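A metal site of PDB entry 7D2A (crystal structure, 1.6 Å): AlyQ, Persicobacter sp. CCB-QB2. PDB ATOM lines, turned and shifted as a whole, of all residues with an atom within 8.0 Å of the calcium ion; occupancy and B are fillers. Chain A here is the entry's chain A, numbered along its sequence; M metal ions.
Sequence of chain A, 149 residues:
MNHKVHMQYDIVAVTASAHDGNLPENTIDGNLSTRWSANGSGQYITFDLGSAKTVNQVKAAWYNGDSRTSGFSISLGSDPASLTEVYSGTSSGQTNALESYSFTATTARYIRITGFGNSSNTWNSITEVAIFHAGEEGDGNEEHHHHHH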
ATOM      1  N   LEU A  23      -5.308   0.066 -18.594  1.00  0.00           N
ATOM      2  CA  LEU A  23      -4.302   0.652 -17.689  1.00  0.00           C
ATOM      3  C   LEU A  23      -4.693   2.056 -17.239  1.00  0.00           C
ATOM      4  O   LEU A  23      -5.168   2.860 -18.022  1.00  0.00           O
ATOM      5  CB  LEU A  23      -2.936   0.687 -18.373  1.00  0.00           C
ATOM      6  CG  LEU A  23      -2.323  -0.678 -18.615  1.00  0.00           C
ATOM      7  CD1 LEU A  23      -1.043  -0.461 -19.399  1.00  0.00           C
ATOM      8  CD2 LEU A  23      -2.120  -1.364 -17.304  1.00  0.00           C
ATOM      9  N   PRO A  24      -4.168   2.470 -16.072  1.00  0.00           N
ATOM     10  CA  PRO A  24      -4.368   3.838 -15.577  1.00  0.00           C
ATOM     11  C   PRO A  24      -3.973   4.928 -16.576  1.00  0.00           C
ATOM     12  O   PRO A  24      -4.697   5.928 -16.790  1.00  0.00           O
ATOM     13  CB  PRO A  24      -3.541   3.821 -14.303  1.00  0.00           C
ATOM     14  CG  PRO A  24      -3.717   2.425 -13.784  1.00  0.00           C
ATOM     15  CD  PRO A  24      -3.571   1.609 -15.031  1.00  0.00           C
ATOM     16  N   GLU A  25      -2.835   4.714 -17.238  1.00  0.00           N
ATOM     17  CA  GLU A  25      -2.246   5.674 -18.200  1.00  0.00           C
ATOM     18  C   GLU A  25      -3.133   5.852 -19.432  1.00  0.00           C
ATOM     19  O   GLU A  25      -2.948   6.813 -20.137  1.00  0.00           O
ATOM     20  CB  GLU A  25      -0.851   5.231 -18.636  1.00  0.00           C
ATOM     21  CG  GLU A  25      -0.822   4.183 -19.735  1.00  0.00           C
ATOM     22  CD  GLU A  25       0.552   3.597 -20.020  1.00  0.00           C
ATOM     23  OE1 GLU A  25       1.568   4.372 -20.117  1.00  0.00           O
ATOM     24  OE2 GLU A  25       0.643   2.394 -20.050  1.00  0.00           O
ATOM     25  N   ASN A  26      -4.100   4.962 -19.646  1.00  0.00           N
ATOM     26  CA  ASN A  26      -5.020   5.161 -20.775  1.00  0.00           C
ATOM     27  C   ASN A  26      -5.869   6.430 -20.588  1.00  0.00           C
ATOM     28  O   ASN A  26      -6.541   6.889 -21.529  1.00  0.00           O
ATOM     29  CB  ASN A  26      -5.928   3.968 -20.969  1.00  0.00           C
ATOM     30  CG  ASN A  26      -5.190   2.768 -21.531  1.00  0.00           C
ATOM     31  OD1 ASN A  26      -4.016   2.831 -21.925  1.00  0.00           O
ATOM     32  ND2 ASN A  26      -5.917   1.671 -21.562  1.00  0.00           N
ATOM     33  N   THR A  27      -5.953   6.965 -19.377  1.00  0.00           N
ATOM     34  CA  THR A  27      -6.742   8.197 -19.118  1.00  0.00           C
ATOM     35  C   THR A  27      -6.033   9.441 -19.588  1.00  0.00           C
ATOM     36  O   THR A  27      -6.665  10.497 -19.592  1.00  0.00           O
ATOM     37  CB  THR A  27      -7.081   8.341 -17.628  1.00  0.00           C
ATOM     38  OG1 THR A  27      -5.886   8.385 -16.859  1.00  0.00           O
ATOM     39  CG2 THR A  27      -7.927   7.195 -17.137  1.00  0.00           C
ATOM     40  N   ILE A  28      -4.770   9.354 -20.004  1.00  0.00           N
ATOM     41  CA  ILE A  28      -4.022  10.590 -20.394  1.00  0.00           C
ATOM     42  C   ILE A  28      -3.423  10.421 -21.782  1.00  0.00           C
ATOM     43  O   ILE A  28      -2.436  11.140 -22.098  1.00  0.00           O
ATOM     44  CB  ILE A  28      -2.998  11.001 -19.329  1.00  0.00           C
ATOM     45  CG1 ILE A  28      -1.926   9.957 -19.106  1.00  0.00           C
ATOM     46  CG2 ILE A  28      -3.700  11.334 -18.012  1.00  0.00           C
ATOM     47  CD1 ILE A  28      -0.715  10.529 -18.348  1.00  0.00           C
ATOM     48  N   ASP A  29      -4.009   9.557 -22.588  1.00  0.00           N
ATOM     49  CA  ASP A  29      -3.455   9.341 -23.944  1.00  0.00           C
ATOM     50  C   ASP A  29      -4.198  10.191 -24.975  1.00  0.00           C
ATOM     51  O   ASP A  29      -3.816  10.128 -26.169  1.00  0.00           O
ATOM     52  CB  ASP A  29      -3.426   7.853 -24.294  1.00  0.00           C
ATOM     53  CG  ASP A  29      -4.786   7.183 -24.417  1.00  0.00           C
ATOM     54  OD1 ASP A  29      -5.832   7.867 -24.226  1.00  0.00           O
ATOM     55  OD2 ASP A  29      -4.761   5.988 -24.764  1.00  0.00           O
ATOM     56  N   GLY A  30      -5.214  10.974 -24.603  1.00  0.00           N
ATOM     57  CA  GLY A  30      -5.944  11.799 -25.561  1.00  0.00           C
ATOM     58  C   GLY A  30      -6.977  11.016 -26.342  1.00  0.00           C
ATOM     59  O   GLY A  30      -7.543  11.548 -27.242  1.00  0.00           O
ATOM     60  N   ASN A  31      -7.165   9.737 -26.047  1.00  0.00           N
ATOM     61  CA  ASN A  31      -8.037   8.848 -26.851  1.00  0.00           C
ATOM     62  C   ASN A  31      -9.288   8.471 -26.045  1.00  0.00           C
ATOM     63  O   ASN A  31      -9.158   7.717 -25.033  1.00  0.00           O
ATOM     64  CB  ASN A  31      -7.256   7.623 -27.253  1.00  0.00           C
ATOM     65  CG  ASN A  31      -7.905   6.855 -28.365  1.00  0.00           C
ATOM     66  OD1 ASN A  31      -9.107   6.951 -28.574  1.00  0.00           O
ATOM     67  ND2 ASN A  31      -7.065   6.081 -29.064  1.00  0.00           N
ATOM     68  N   LEU A  32     -10.462   8.838 -26.560  1.00  0.00           N
ATOM     69  CA  LEU A  32     -11.728   8.470 -25.879  1.00  0.00           C
ATOM     70  C   LEU A  32     -12.022   6.986 -26.071  1.00  0.00           C
ATOM     71  O   LEU A  32     -12.950   6.507 -25.399  1.00  0.00           O
ATOM     72  CB  LEU A  32     -12.887   9.343 -26.359  1.00  0.00           C
ATOM     73  CG  LEU A  32     -12.780  10.832 -25.991  1.00  0.00           C
ATOM     74  CD1 LEU A  32     -13.724  11.641 -26.812  1.00  0.00           C
ATOM     75  CD2 LEU A  32     -13.088  11.032 -24.518  1.00  0.00           C
ATOM     76  N   SER A  33     -11.291   6.251 -26.914  1.00  0.00           N
ATOM     77  CA  SER A  33     -11.555   4.800 -27.132  1.00  0.00           C
ATOM     78  C   SER A  33     -10.713   3.925 -26.200  1.00  0.00           C
ATOM     79  O   SER A  33     -10.864   2.684 -26.284  1.00  0.00           O
ATOM     80  CB  SER A  33     -11.330   4.401 -28.577  1.00  0.00           C
ATOM     81  OG  SER A  33      -9.951   4.301 -28.871  1.00  0.00           O
ATOM     82  N   THR A  34      -9.864   4.523 -25.366  1.00  0.00           N
ATOM     83  CA  THR A  34      -9.039   3.751 -24.412  1.00  0.00           C
ATOM     84  C   THR A  34      -9.389   4.196 -23.009  1.00  0.00           C
ATOM     85  O   THR A  34      -9.656   5.410 -22.810  1.00  0.00           O
ATOM     86  CB  THR A  34      -7.562   3.945 -24.677  1.00  0.00           C
ATOM     87  OG1 THR A  34      -7.289   5.308 -24.379  1.00  0.00           O
ATOM     88  CG2 THR A  34      -7.174   3.549 -26.093  1.00  0.00           C
ATOM     89  N   ARG A  35      -9.392   3.263 -22.066  1.00  0.00           N
ATOM     90  CA  ARG A  35      -9.918   3.536 -20.718  1.00  0.00           C
ATOM     91  C   ARG A  35      -9.011   2.912 -19.655  1.00  0.00           C
ATOM     92  O   ARG A  35      -8.256   1.962 -19.932  1.00  0.00           O
ATOM     93  CB  ARG A  35     -11.320   2.962 -20.524  1.00  0.00           C
ATOM     94  CG  ARG A  35     -11.391   1.456 -20.532  1.00  0.00           C
ATOM     95  CD  ARG A  35     -12.823   0.958 -20.544  1.00  0.00           C
ATOM     96  NE  ARG A  35     -12.901  -0.488 -20.487  1.00  0.00           N
ATOM     97  CZ  ARG A  35     -13.008  -1.299 -21.539  1.00  0.00           C
ATOM     98  NH1 ARG A  35     -13.013  -0.818 -22.780  1.00  0.00           N
ATOM     99  NH2 ARG A  35     -13.140  -2.606 -21.349  1.00  0.00           N
ATOM    100  N   TRP A  36      -9.174   3.417 -18.427  1.00  0.00           N
ATOM    101  CA  TRP A  36      -8.814   2.658 -17.219  1.00  0.00           C
ATOM    102  C   TRP A  36     -10.090   2.010 -16.688  1.00  0.00           C
ATOM    103  O   TRP A  36     -11.155   2.698 -16.655  1.00  0.00           O
ATOM    104  CB  TRP A  36      -8.292   3.635 -16.162  1.00  0.00           C
ATOM    105  CG  TRP A  36      -8.255   3.062 -14.778  1.00  0.00           C
ATOM    106  CD1 TRP A  36      -7.462   2.064 -14.322  1.00  0.00           C
ATOM    107  CD2 TRP A  36      -9.079   3.445 -13.675  1.00  0.00           C
ATOM    108  NE1 TRP A  36      -7.700   1.800 -13.008  1.00  0.00           N
ATOM    109  CE2 TRP A  36      -8.693   2.643 -12.570  1.00  0.00           C
ATOM    110  CE3 TRP A  36     -10.080   4.408 -13.493  1.00  0.00           C
ATOM    111  CZ2 TRP A  36      -9.262   2.782 -11.296  1.00  0.00           C
ATOM    112  CZ3 TRP A  36     -10.691   4.497 -12.260  1.00  0.00           C
ATOM    113  CH2 TRP A  36     -10.258   3.724 -11.163  1.00  0.00           C
ATOM    114  N   ALA A  61     -13.842  12.107 -18.719  1.00  0.00           N
ATOM    115  CA  ALA A  61     -14.700  11.440 -19.719  1.00  0.00           C
ATOM    116  C   ALA A  61     -14.911  10.020 -19.264  1.00  0.00           C
ATOM    117  O   ALA A  61     -13.946   9.300 -18.953  1.00  0.00           O
ATOM    118  CB  ALA A  61     -14.067  11.517 -21.096  1.00  0.00           C
ATOM    119  N   ILE A 126     -12.989   5.008 -16.926  1.00  0.00           N
ATOM    120  CA  ILE A 126     -12.719   6.411 -17.271  1.00  0.00           C
ATOM    121  C   ILE A 126     -11.885   6.419 -18.541  1.00  0.00           C
ATOM    122  O   ILE A 126     -10.825   5.770 -18.548  1.00  0.00           O
ATOM    123  CB  ILE A 126     -12.068   7.181 -16.104  1.00  0.00           C
ATOM    124  CG1 ILE A 126     -12.993   7.123 -14.863  1.00  0.00           C
ATOM    125  CG2 ILE A 126     -11.733   8.587 -16.544  1.00  0.00           C
ATOM    126  CD1 ILE A 126     -12.377   7.765 -13.628  1.00  0.00           C
ATOM    127  N   THR A 127     -12.317   7.180 -19.572  1.00  0.00           N
ATOM    128  CA  THR A 127     -11.537   7.202 -20.820  1.00  0.00           C
ATOM    129  C   THR A 127     -10.486   8.303 -20.850  1.00  0.00           C
ATOM    130  O   THR A 127      -9.408   8.089 -21.449  1.00  0.00           O
ATOM    131  CB  THR A 127     -12.476   7.312 -22.020  1.00  0.00           C
ATOM    132  OG1 THR A 127     -13.180   8.549 -21.892  1.00  0.00           O
ATOM    133  CG2 THR A 127     -13.458   6.161 -22.107  1.00  0.00           C
ATOM    134  N   GLU A 128     -10.725   9.444 -20.232  1.00  0.00           N
ATOM    135  CA  GLU A 128      -9.789  10.589 -20.269  1.00  0.00           C
ATOM    136  C   GLU A 128      -9.937  11.375 -18.986  1.00  0.00           C
ATOM    137  O   GLU A 128     -11.110  11.539 -18.547  1.00  0.00           O
ATOM    138  CB  GLU A 128     -10.093  11.462 -21.492  1.00  0.00           C
ATOM    139  CG  GLU A 128      -9.621  10.847 -22.815  1.00  0.00           C
ATOM    140  CD  GLU A 128      -8.110  10.728 -22.885  1.00  0.00           C
ATOM    141  OE1 GLU A 128      -7.442  11.817 -22.897  1.00  0.00           O
ATOM    142  OE2 GLU A 128      -7.541   9.594 -22.960  1.00  0.00           O
ATOM    143  N   VAL A 129      -8.837  11.932 -18.494  1.00  0.00           N
ATOM    144  CA  VAL A 129      -8.868  12.929 -17.401  1.00  0.00           C
ATOM    145  C   VAL A 129      -7.967  14.087 -17.776  1.00  0.00           C
ATOM    146  O   VAL A 129      -6.858  13.825 -18.323  1.00  0.00           O
ATOM    147  CB  VAL A 129      -8.457  12.290 -16.071  1.00  0.00           C
ATOM    148  CG1 VAL A 129      -8.276  13.347 -14.970  1.00  0.00           C
ATOM    149  CG2 VAL A 129      -9.469  11.286 -15.597  1.00  0.00           C
HETATM  150 CA    CA M   1      -7.993   7.281 -23.154  1.00  0.00          CA
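Six residues have an atom within 4 Å of the calcium ion: Asn 26, Asp 29, Asn 31, Thr 34, Thr 127 and Glu 128.
N of Ala 61 is in hydrogen-bond range of O of Glu 128 (2.8 Å). N of Gly 30 is in hydrogen-bond range of OE1 of Glu 128, at 2.9 Å. The backbone NH (N) of Thr 127 sits at hydrogen-bond distance from the backbone carbonyl oxygen (O) of Ala 61, 2.7 Å away. ND2 of Asn 26 sits at hydrogen-bond distance from O of Arg 35, at 2.9 Å. The side-chain hydroxyl (OG) of Ser 33 sits at hydrogen-bond distance from the side-chain amide oxygen (OD1) of Asn 31, at 2.8 Å. The side-chain amide nitrogen (ND2) of Asn 26 lies close to the backbone NH (N) of Leu 23, 3.4 Å away.
The calcium ion is bound by O of Asn 26, O of Asn 31, O of Thr 127, OE2 of Glu 128, OG1 of Thr 34, OD1 of Asp 29 and O of Thr 34.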
